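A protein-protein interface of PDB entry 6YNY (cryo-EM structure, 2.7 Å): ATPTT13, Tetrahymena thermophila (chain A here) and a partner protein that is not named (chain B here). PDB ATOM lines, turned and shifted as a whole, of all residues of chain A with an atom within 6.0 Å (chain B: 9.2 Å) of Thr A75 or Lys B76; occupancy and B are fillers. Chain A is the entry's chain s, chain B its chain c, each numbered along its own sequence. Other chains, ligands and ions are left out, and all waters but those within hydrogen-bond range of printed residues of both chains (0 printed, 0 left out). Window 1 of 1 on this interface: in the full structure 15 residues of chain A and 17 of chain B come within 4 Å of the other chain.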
ATOM      1  N   MET A  63     -11.842  13.230 -19.527  1.00  0.00           N
ATOM      2  CA  MET A  63     -11.972  12.392 -20.703  1.00  0.00           C
ATOM      3  C   MET A  63     -13.219  11.520 -20.606  1.00  0.00           C
ATOM      4  O   MET A  63     -13.743  11.251 -19.523  1.00  0.00           O
ATOM      5  CB  MET A  63     -10.729  11.525 -20.880  1.00  0.00           C
ATOM      6  CG  MET A  63      -9.486  12.323 -21.220  1.00  0.00           C
ATOM      7  SD  MET A  63      -7.996  11.328 -21.374  1.00  0.00           S
ATOM      8  CE  MET A  63      -8.368  10.409 -22.859  1.00  0.00           C
ATOM      9  N   LEU A  67     -14.087   5.442 -23.519  1.00  0.00           N
ATOM     10  CA  LEU A  67     -12.753   4.926 -23.813  1.00  0.00           C
ATOM     11  C   LEU A  67     -12.309   4.024 -22.661  1.00  0.00           C
ATOM     12  O   LEU A  67     -11.408   4.341 -21.883  1.00  0.00           O
ATOM     13  CB  LEU A  67     -11.788   6.084 -24.021  1.00  0.00           C
ATOM     14  CG  LEU A  67     -11.879   6.913 -25.304  1.00  0.00           C
ATOM     15  CD1 LEU A  67     -13.285   7.035 -25.822  1.00  0.00           C
ATOM     16  CD2 LEU A  67     -11.335   8.297 -25.036  1.00  0.00           C
ATOM     17  N   ASP A  73      -5.955  -0.801 -31.839  1.00  0.00           N
ATOM     18  CA  ASP A  73      -6.433  -0.438 -33.166  1.00  0.00           C
ATOM     19  C   ASP A  73      -5.484   0.595 -33.760  1.00  0.00           C
ATOM     20  O   ASP A  73      -4.384   0.823 -33.250  1.00  0.00           O
ATOM     21  CB  ASP A  73      -7.880   0.067 -33.103  1.00  0.00           C
ATOM     22  CG  ASP A  73      -8.034   1.298 -32.240  1.00  0.00           C
ATOM     23  OD1 ASP A  73      -7.040   1.725 -31.620  1.00  0.00           O
ATOM     24  OD2 ASP A  73      -9.153   1.844 -32.182  1.00  0.00           O
ATOM     25  N   ASP A  74      -5.920   1.223 -34.853  1.00  0.00           N
ATOM     26  CA  ASP A  74      -5.056   2.146 -35.576  1.00  0.00           C
ATOM     27  C   ASP A  74      -4.800   3.425 -34.791  1.00  0.00           C
ATOM     28  O   ASP A  74      -3.756   4.059 -34.971  1.00  0.00           O
ATOM     29  CB  ASP A  74      -5.671   2.480 -36.934  1.00  0.00           C
ATOM     30  CG  ASP A  74      -5.764   1.279 -37.845  1.00  0.00           C
ATOM     31  OD1 ASP A  74      -4.809   0.478 -37.879  1.00  0.00           O
ATOM     32  OD2 ASP A  74      -6.795   1.138 -38.534  1.00  0.00           O
ATOM     33  N   THR A  75      -5.734   3.827 -33.929  1.00  0.00           N
ATOM     34  CA  THR A  75      -5.555   5.057 -33.167  1.00  0.00           C
ATOM     35  C   THR A  75      -4.359   4.985 -32.233  1.00  0.00           C
ATOM     36  O   THR A  75      -3.869   6.028 -31.791  1.00  0.00           O
ATOM     37  CB  THR A  75      -6.808   5.367 -32.351  1.00  0.00           C
ATOM     38  OG1 THR A  75      -7.022   4.332 -31.387  1.00  0.00           O
ATOM     39  CG2 THR A  75      -8.008   5.463 -33.247  1.00  0.00           C
ATOM     40  N   ASN A  76      -3.880   3.784 -31.922  1.00  0.00           N
ATOM     41  CA  ASN A  76      -2.774   3.651 -30.985  1.00  0.00           C
ATOM     42  C   ASN A  76      -1.452   4.044 -31.626  1.00  0.00           C
ATOM     43  O   ASN A  76      -0.654   4.756 -31.010  1.00  0.00           O
ATOM     44  CB  ASN A  76      -2.713   2.225 -30.454  1.00  0.00           C
ATOM     45  CG  ASN A  76      -3.985   1.816 -29.754  1.00  0.00           C
ATOM     46  OD1 ASN A  76      -4.833   1.134 -30.324  1.00  0.00           O
ATOM     47  ND2 ASN A  76      -4.128   2.237 -28.510  1.00  0.00           N
ATOM     48  N   TRP A  77      -1.195   3.597 -32.856  1.00  0.00           N
ATOM     49  CA  TRP A  77       0.046   3.964 -33.518  1.00  0.00           C
ATOM     50  C   TRP A  77      -0.007   5.364 -34.102  1.00  0.00           C
ATOM     51  O   TRP A  77       1.044   5.987 -34.274  1.00  0.00           O
ATOM     52  CB  TRP A  77       0.402   2.952 -34.610  1.00  0.00           C
ATOM     53  CG  TRP A  77      -0.564   2.826 -35.752  1.00  0.00           C
ATOM     54  CD1 TRP A  77      -1.474   1.834 -35.938  1.00  0.00           C
ATOM     55  CD2 TRP A  77      -0.693   3.702 -36.879  1.00  0.00           C
ATOM     56  NE1 TRP A  77      -2.166   2.037 -37.101  1.00  0.00           N
ATOM     57  CE2 TRP A  77      -1.708   3.179 -37.697  1.00  0.00           C
ATOM     58  CE3 TRP A  77      -0.052   4.877 -37.273  1.00  0.00           C
ATOM     59  CZ2 TRP A  77      -2.101   3.791 -38.880  1.00  0.00           C
ATOM     60  CZ3 TRP A  77      -0.446   5.484 -38.445  1.00  0.00           C
ATOM     61  CH2 TRP A  77      -1.458   4.940 -39.236  1.00  0.00           C
ATOM     62  N   TYR A  78      -1.199   5.876 -34.400  1.00  0.00           N
ATOM     63  CA  TYR A  78      -1.303   7.239 -34.902  1.00  0.00           C
ATOM     64  C   TYR A  78      -1.053   8.245 -33.791  1.00  0.00           C
ATOM     65  O   TYR A  78      -0.386   9.264 -34.003  1.00  0.00           O
ATOM     66  CB  TYR A  78      -2.675   7.463 -35.531  1.00  0.00           C
ATOM     67  CG  TYR A  78      -2.843   8.831 -36.134  1.00  0.00           C
ATOM     68  CD1 TYR A  78      -2.362   9.112 -37.401  1.00  0.00           C
ATOM     69  CD2 TYR A  78      -3.479   9.843 -35.440  1.00  0.00           C
ATOM     70  CE1 TYR A  78      -2.509  10.356 -37.952  1.00  0.00           C
ATOM     71  CE2 TYR A  78      -3.630  11.090 -35.986  1.00  0.00           C
ATOM     72  CZ  TYR A  78      -3.145  11.342 -37.244  1.00  0.00           C
ATOM     73  OH  TYR A  78      -3.287  12.585 -37.801  1.00  0.00           O
ATOM     74  N   GLN A  79      -1.581   7.972 -32.600  1.00  0.00           N
ATOM     75  CA  GLN A  79      -1.343   8.847 -31.461  1.00  0.00           C
ATOM     76  C   GLN A  79       0.067   8.684 -30.918  1.00  0.00           C
ATOM     77  O   GLN A  79       0.628   9.633 -30.360  1.00  0.00           O
ATOM     78  CB  GLN A  79      -2.367   8.560 -30.369  1.00  0.00           C
ATOM     79  CG  GLN A  79      -2.406   9.587 -29.279  1.00  0.00           C
ATOM     80  CD  GLN A  79      -3.519   9.345 -28.298  1.00  0.00           C
ATOM     81  OE1 GLN A  79      -3.683   8.240 -27.786  1.00  0.00           O
ATOM     82  NE2 GLN A  79      -4.300  10.376 -28.033  1.00  0.00           N
ATOM     83  N   ALA A  80       0.654   7.499 -31.072  1.00  0.00           N
ATOM     84  CA  ALA A  80       2.030   7.292 -30.640  1.00  0.00           C
ATOM     85  C   ALA A  80       2.988   8.167 -31.433  1.00  0.00           C
ATOM     86  O   ALA A  80       3.876   8.813 -30.864  1.00  0.00           O
ATOM     87  CB  ALA A  80       2.399   5.819 -30.784  1.00  0.00           C
ATOM     88  N   PHE B  67     -14.792  -2.641 -31.297  1.00  0.00           N
ATOM     89  CA  PHE B  67     -14.184  -1.759 -32.277  1.00  0.00           C
ATOM     90  C   PHE B  67     -14.523  -0.309 -31.977  1.00  0.00           C
ATOM     91  O   PHE B  67     -15.626   0.008 -31.526  1.00  0.00           O
ATOM     92  CB  PHE B  67     -14.644  -2.124 -33.684  1.00  0.00           C
ATOM     93  CG  PHE B  67     -14.208  -3.484 -34.123  1.00  0.00           C
ATOM     94  CD1 PHE B  67     -12.939  -3.687 -34.626  1.00  0.00           C
ATOM     95  CD2 PHE B  67     -15.064  -4.561 -34.025  1.00  0.00           C
ATOM     96  CE1 PHE B  67     -12.537  -4.934 -35.025  1.00  0.00           C
ATOM     97  CE2 PHE B  67     -14.664  -5.810 -34.424  1.00  0.00           C
ATOM     98  CZ  PHE B  67     -13.398  -5.997 -34.923  1.00  0.00           C
ATOM     99  N   ARG B  68     -13.557   0.566 -32.225  1.00  0.00           N
ATOM    100  CA  ARG B  68     -13.719   1.976 -31.916  1.00  0.00           C
ATOM    101  C   ARG B  68     -14.669   2.636 -32.906  1.00  0.00           C
ATOM    102  O   ARG B  68     -14.659   2.330 -34.100  1.00  0.00           O
ATOM    103  CB  ARG B  68     -12.361   2.668 -31.941  1.00  0.00           C
ATOM    104  CG  ARG B  68     -12.329   3.999 -31.245  1.00  0.00           C
ATOM    105  CD  ARG B  68     -10.921   4.540 -31.185  1.00  0.00           C
ATOM    106  NE  ARG B  68     -10.039   3.687 -30.398  1.00  0.00           N
ATOM    107  CZ  ARG B  68      -9.843   3.809 -29.089  1.00  0.00           C
ATOM    108  NH1 ARG B  68     -10.465   4.748 -28.395  1.00  0.00           N
ATOM    109  NH2 ARG B  68      -9.020   2.982 -28.470  1.00  0.00           N
ATOM    110  N   THR B  69     -15.499   3.542 -32.399  1.00  0.00           N
ATOM    111  CA  THR B  69     -16.433   4.278 -33.233  1.00  0.00           C
ATOM    112  C   THR B  69     -15.823   5.610 -33.659  1.00  0.00           C
ATOM    113  O   THR B  69     -14.720   5.980 -33.253  1.00  0.00           O
ATOM    114  CB  THR B  69     -17.751   4.500 -32.497  1.00  0.00           C
ATOM    115  OG1 THR B  69     -17.520   5.267 -31.311  1.00  0.00           O
ATOM    116  CG2 THR B  69     -18.380   3.181 -32.124  1.00  0.00           C
ATOM    117  N   TYR B  70     -16.557   6.346 -34.491  1.00  0.00           N
ATOM    118  CA  TYR B  70     -16.080   7.644 -34.956  1.00  0.00           C
ATOM    119  C   TYR B  70     -15.823   8.582 -33.786  1.00  0.00           C
ATOM    120  O   TYR B  70     -14.758   9.199 -33.689  1.00  0.00           O
ATOM    121  CB  TYR B  70     -17.095   8.255 -35.920  1.00  0.00           C
ATOM    122  CG  TYR B  70     -16.679   9.594 -36.479  1.00  0.00           C
ATOM    123  CD1 TYR B  70     -16.021   9.683 -37.691  1.00  0.00           C
ATOM    124  CD2 TYR B  70     -16.941  10.768 -35.792  1.00  0.00           C
ATOM    125  CE1 TYR B  70     -15.638  10.898 -38.203  1.00  0.00           C
ATOM    126  CE2 TYR B  70     -16.559  11.985 -36.295  1.00  0.00           C
ATOM    127  CZ  TYR B  70     -15.905  12.046 -37.502  1.00  0.00           C
ATOM    128  OH  TYR B  70     -15.521  13.260 -38.015  1.00  0.00           O
ATOM    129  N   THR B  71     -16.800   8.706 -32.889  1.00  0.00           N
ATOM    130  CA  THR B  71     -16.655   9.607 -31.754  1.00  0.00           C
ATOM    131  C   THR B  71     -15.501   9.189 -30.856  1.00  0.00           C
ATOM    132  O   THR B  71     -14.762  10.038 -30.346  1.00  0.00           O
ATOM    133  CB  THR B  71     -17.956   9.654 -30.961  1.00  0.00           C
ATOM    134  OG1 THR B  71     -18.334   8.326 -30.584  1.00  0.00           O
ATOM    135  CG2 THR B  71     -19.049  10.277 -31.793  1.00  0.00           C
ATOM    136  N   GLU B  72     -15.327   7.885 -30.652  1.00  0.00           N
ATOM    137  CA  GLU B  72     -14.236   7.408 -29.816  1.00  0.00           C
ATOM    138  C   GLU B  72     -12.876   7.645 -30.455  1.00  0.00           C
ATOM    139  O   GLU B  72     -11.869   7.683 -29.744  1.00  0.00           O
ATOM    140  CB  GLU B  72     -14.430   5.924 -29.514  1.00  0.00           C
ATOM    141  CG  GLU B  72     -15.682   5.619 -28.724  1.00  0.00           C
ATOM    142  CD  GLU B  72     -15.943   4.137 -28.577  1.00  0.00           C
ATOM    143  OE1 GLU B  72     -15.216   3.336 -29.197  1.00  0.00           O
ATOM    144  OE2 GLU B  72     -16.882   3.773 -27.841  1.00  0.00           O
ATOM    145  N   VAL B  73     -12.827   7.811 -31.777  1.00  0.00           N
ATOM    146  CA  VAL B  73     -11.577   8.139 -32.448  1.00  0.00           C
ATOM    147  C   VAL B  73     -11.237   9.610 -32.260  1.00  0.00           C
ATOM    148  O   VAL B  73     -10.095   9.966 -31.951  1.00  0.00           O
ATOM    149  CB  VAL B  73     -11.671   7.769 -33.939  1.00  0.00           C
ATOM    150  CG1 VAL B  73     -10.520   8.353 -34.707  1.00  0.00           C
ATOM    151  CG2 VAL B  73     -11.698   6.275 -34.115  1.00  0.00           C
ATOM    152  N   LEU B  74     -12.224  10.487 -32.441  1.00  0.00           N
ATOM    153  CA  LEU B  74     -11.979  11.918 -32.300  1.00  0.00           C
ATOM    154  C   LEU B  74     -11.633  12.290 -30.866  1.00  0.00           C
ATOM    155  O   LEU B  74     -10.807  13.179 -30.632  1.00  0.00           O
ATOM    156  CB  LEU B  74     -13.203  12.703 -32.767  1.00  0.00           C
ATOM    157  CG  LEU B  74     -13.256  13.114 -34.234  1.00  0.00           C
ATOM    158  CD1 LEU B  74     -12.195  14.157 -34.505  1.00  0.00           C
ATOM    159  CD2 LEU B  74     -13.087  11.921 -35.148  1.00  0.00           C
ATOM    160  N   LEU B  75     -12.257  11.627 -29.895  1.00  0.00           N
ATOM    161  CA  LEU B  75     -12.013  11.965 -28.498  1.00  0.00           C
ATOM    162  C   LEU B  75     -10.617  11.551 -28.056  1.00  0.00           C
ATOM    163  O   LEU B  75      -9.947  12.289 -27.327  1.00  0.00           O
ATOM    164  CB  LEU B  75     -13.066  11.302 -27.620  1.00  0.00           C
ATOM    165  CG  LEU B  75     -14.478  11.869 -27.752  1.00  0.00           C
ATOM    166  CD1 LEU B  75     -15.480  10.972 -27.080  1.00  0.00           C
ATOM    167  CD2 LEU B  75     -14.543  13.252 -27.161  1.00  0.00           C
ATOM    168  N   LYS B  76     -10.160  10.378 -28.487  1.00  0.00           N
ATOM    169  CA  LYS B  76      -8.846   9.903 -28.077  1.00  0.00           C
ATOM    170  C   LYS B  76      -7.726  10.746 -28.672  1.00  0.00           C
ATOM    171  O   LYS B  76      -6.685  10.930 -28.032  1.00  0.00           O
ATOM    172  CB  LYS B  76      -8.680   8.442 -28.484  1.00  0.00           C
ATOM    173  CG  LYS B  76      -7.295   7.871 -28.274  1.00  0.00           C
ATOM    174  CD  LYS B  76      -7.217   6.456 -28.784  1.00  0.00           C
ATOM    175  CE  LYS B  76      -5.816   5.902 -28.694  1.00  0.00           C
ATOM    176  NZ  LYS B  76      -5.293   5.964 -27.321  1.00  0.00           N
ATOM    177  N   ILE B  77      -7.919  11.268 -29.877  1.00  0.00           N
ATOM    178  CA  ILE B  77      -6.844  11.901 -30.629  1.00  0.00           C
ATOM    179  C   ILE B  77      -6.923  13.418 -30.534  1.00  0.00           C
ATOM    180  O   ILE B  77      -5.896  14.103 -30.574  1.00  0.00           O
ATOM    181  CB  ILE B  77      -6.877  11.436 -32.093  1.00  0.00           C
ATOM    182  CG1 ILE B  77      -6.456   9.971 -32.179  1.00  0.00           C
ATOM    183  CG2 ILE B  77      -5.987  12.304 -32.947  1.00  0.00           C
ATOM    184  CD1 ILE B  77      -6.811   9.312 -33.467  1.00  0.00           C
ATOM    185  N   SER B  78      -8.135  13.957 -30.413  1.00  0.00           N
ATOM    186  CA  SER B  78      -8.328  15.400 -30.421  1.00  0.00           C
ATOM    187  C   SER B  78      -9.096  15.906 -29.208  1.00  0.00           C
ATOM    188  O   SER B  78      -9.549  17.055 -29.216  1.00  0.00           O
ATOM    189  CB  SER B  78      -9.049  15.834 -31.698  1.00  0.00           C
ATOM    190  OG  SER B  78      -9.053  17.240 -31.814  1.00  0.00           O
ATOM    191  N   ALA B  79      -9.258  15.087 -28.168  1.00  0.00           N
ATOM    192  CA  ALA B  79      -9.922  15.544 -26.954  1.00  0.00           C
ATOM    193  C   ALA B  79      -9.224  15.032 -25.701  1.00  0.00           C
ATOM    194  O   ALA B  79      -9.837  15.005 -24.629  1.00  0.00           O
ATOM    195  CB  ALA B  79     -11.382  15.115 -26.925  1.00  0.00           C
ATOM    196  N   TYR B  80      -7.966  14.624 -25.807  1.00  0.00           N
ATOM    197  CA  TYR B  80      -7.235  14.163 -24.641  1.00  0.00           C
ATOM    198  C   TYR B  80      -6.867  15.340 -23.748  1.00  0.00           C
ATOM    199  O   TYR B  80      -6.651  16.462 -24.213  1.00  0.00           O
ATOM    200  CB  TYR B  80      -5.979  13.406 -25.059  1.00  0.00           C
ATOM    201  CG  TYR B  80      -4.985  14.219 -25.850  1.00  0.00           C
ATOM    202  CD1 TYR B  80      -4.058  15.025 -25.216  1.00  0.00           C
ATOM    203  CD2 TYR B  80      -4.961  14.164 -27.230  1.00  0.00           C
ATOM    204  CE1 TYR B  80      -3.148  15.760 -25.934  1.00  0.00           C
ATOM    205  CE2 TYR B  80      -4.055  14.895 -27.953  1.00  0.00           C
ATOM    206  CZ  TYR B  80      -3.149  15.689 -27.300  1.00  0.00           C
ATOM    207  OH  TYR B  80      -2.243  16.422 -28.022  1.00  0.00           O
ATOM    208  N   ASN B  81      -6.808  15.072 -22.451  1.00  0.00           N
ATOM    209  CA  ASN B  81      -6.547  16.105 -21.465  1.00  0.00           C
ATOM    210  C   ASN B  81      -5.045  16.209 -21.214  1.00  0.00           C
ATOM    211  O   ASN B  81      -4.230  15.573 -21.887  1.00  0.00           O
ATOM    212  CB  ASN B  81      -7.321  15.814 -20.184  1.00  0.00           C
ATOM    213  CG  ASN B  81      -6.939  14.495 -19.556  1.00  0.00           C
ATOM    214  OD1 ASN B  81      -5.934  13.887 -19.914  1.00  0.00           O
ATOM    215  ND2 ASN B  81      -7.744  14.045 -18.610  1.00  0.00           N
ATOM    216  N   PHE B  84      -3.370  12.884 -19.657  1.00  0.00           N
ATOM    217  CA  PHE B  84      -3.104  11.851 -20.651  1.00  0.00           C
ATOM    218  C   PHE B  84      -1.846  12.165 -21.447  1.00  0.00           C
ATOM    219  O   PHE B  84      -1.016  11.281 -21.686  1.00  0.00           O
ATOM    220  CB  PHE B  84      -4.306  11.711 -21.578  1.00  0.00           C
ATOM    221  CG  PHE B  84      -4.189  10.588 -22.553  1.00  0.00           C
ATOM    222  CD1 PHE B  84      -3.688  10.803 -23.819  1.00  0.00           C
ATOM    223  CD2 PHE B  84      -4.582   9.313 -22.205  1.00  0.00           C
ATOM    224  CE1 PHE B  84      -3.580   9.772 -24.714  1.00  0.00           C
ATOM    225  CE2 PHE B  84      -4.475   8.281 -23.098  1.00  0.00           C
ATOM    226  CZ  PHE B  84      -3.974   8.509 -24.353  1.00  0.00           C
ATOM    227  N   TYR B  85      -1.690  13.419 -21.868  1.00  0.00           N
ATOM    228  CA  TYR B  85      -0.495  13.820 -22.600  1.00  0.00           C
ATOM    229  C   TYR B  85       0.757  13.624 -21.758  1.00  0.00           C
ATOM    230  O   TYR B  85       1.814  13.251 -22.278  1.00  0.00           O
ATOM    231  CB  TYR B  85      -0.634  15.278 -23.030  1.00  0.00           C
ATOM    232  CG  TYR B  85       0.584  15.871 -23.686  1.00  0.00           C
ATOM    233  CD1 TYR B  85       0.810  15.713 -25.041  1.00  0.00           C
ATOM    234  CD2 TYR B  85       1.497  16.607 -22.954  1.00  0.00           C
ATOM    235  CE1 TYR B  85       1.916  16.260 -25.646  1.00  0.00           C
ATOM    236  CE2 TYR B  85       2.607  17.158 -23.549  1.00  0.00           C
ATOM    237  CZ  TYR B  85       2.811  16.983 -24.897  1.00  0.00           C
ATOM    238  OH  TYR B  85       3.918  17.531 -25.500  1.00  0.00           O
ATOM    239  N   ASN B  88       1.705   9.564 -21.291  1.00  0.00           N
ATOM    240  CA  ASN B  88       2.366   8.942 -22.431  1.00  0.00           C
ATOM    241  C   ASN B  88       3.819   9.387 -22.535  1.00  0.00           C
ATOM    242  O   ASN B  88       4.730   8.558 -22.628  1.00  0.00           O
ATOM    243  CB  ASN B  88       1.613   9.270 -23.716  1.00  0.00           C
ATOM    244  CG  ASN B  88       0.309   8.522 -23.833  1.00  0.00           C
ATOM    245  OD1 ASN B  88       0.209   7.539 -24.563  1.00  0.00           O
ATOM    246  ND2 ASN B  88      -0.699   8.981 -23.110  1.00  0.00           N
ATOM    247  N   TYR B  92       7.180   7.247 -22.206  1.00  0.00           N
ATOM    248  CA  TYR B  92       8.133   7.216 -23.309  1.00  0.00           C
ATOM    249  C   TYR B  92       9.527   7.611 -22.846  1.00  0.00           C
ATOM    250  O   TYR B  92      10.512   6.938 -23.167  1.00  0.00           O
ATOM    251  CB  TYR B  92       7.665   8.141 -24.430  1.00  0.00           C
ATOM    252  CG  TYR B  92       6.429   7.681 -25.166  1.00  0.00           C
ATOM    253  CD1 TYR B  92       5.786   6.502 -24.831  1.00  0.00           C
ATOM    254  CD2 TYR B  92       5.910   8.428 -26.210  1.00  0.00           C
ATOM    255  CE1 TYR B  92       4.665   6.086 -25.505  1.00  0.00           C
ATOM    256  CE2 TYR B  92       4.790   8.019 -26.890  1.00  0.00           C
ATOM    257  CZ  TYR B  92       4.171   6.849 -26.535  1.00  0.00           C
ATOM    258  OH  TYR B  92       3.050   6.441 -27.217  1.00  0.00           O
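OD1 of Asn B81 lies close to SD of Met A63, at 3.6 Å.
The guanidinium group of Arg B68 lies within salt-bridge range of the side-chain carboxylate of Asp A73.
The guanidinium group (NE) of Arg B68 lies within hydrogen-bond range of the side-chain hydroxyl (OG1) of Thr A75, at 3.2 Å.
O of Lys B76 sits at hydrogen-bond distance from NE2 of Gln A79 (2.4 Å).
OG1 of Thr A75 sits at hydrogen-bond distance from OD1 of Asp A73, 2.6 Å away.
The side-chain carboxylate (OD1) of Asp A73 lies close to the side-chain amide oxygen (OD1) of Asn A76 (2.6 Å).
N of Tyr B80 lies within hydrogen-bond range of O of Leu B75 (3.4 Å).
The side-chain amide oxygen of Asn B81 lies within hydrogen-bond range of the backbone NH of Phe B84 (2.8 Å).
ND2 of Asn B88 is in hydrogen-bond range of O of Phe B84, 2.7 Å away.
Among the printed residues, pairs that only touch across the chains: Met A63 with Phe B84 (3.7 Å), Thr A75 with Val B73 (3.9 Å), Thr A75 with Lys B76 (3.3 Å), Tyr A78 with Ile B77 (3.9 Å), Gln A79 with Ile B77 (3.9 Å), Gln A79 with Tyr B80 (3.9 Å), Gln A79 with Phe B84 (3.4 Å) and Ala A80 with Tyr B92 (3.7 Å).
Thr A75 touches just these residues of chain B: Arg B68 (3.2 Å), Val B73 (3.9 Å) and Lys B76 (3.3 Å).
Lys B76 touches just these residues of chain A: Thr A75 (3.3 Å) and Gln A79 (2.4 Å).
No residue of chain B comes within 4 Å of Asn A76.
Of the printed residues of chain A, Arg B68 touches Asp A73 and Thr A75.
Of the printed residues of chain B, Tyr A78 touches Ile B77 (3.9 Å).
Tyr B85 touches none of the printed residues of chain A.
The nearest residue of chain B that does not touch Thr A75 is Ile B77 (4.04 Å).
Of the 10 printed residues of chain A, 6 touch a printed residue of chain B.
Printed residues of chain A that touch a printed residue of chain B: Met A63, Asp A73, Thr A75, Tyr A78, Gln A79 and Ala A80.
Of the 19 printed residues of chain B, 8 touch a printed residue of chain A.
Hydrophobic or aromatic side chains of chain B within 4 Å of the printed part of chain A: Val B73, Ile B77, Tyr B80, Phe B84 and Tyr B92.
Among the printed residues, 12 pairs touch across the chains.
Among the printed residues, Asp or Glu carboxylates within 4 Å of a Lys or Arg side-chain nitrogen of the other chain: Asp A73 with Arg B68.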
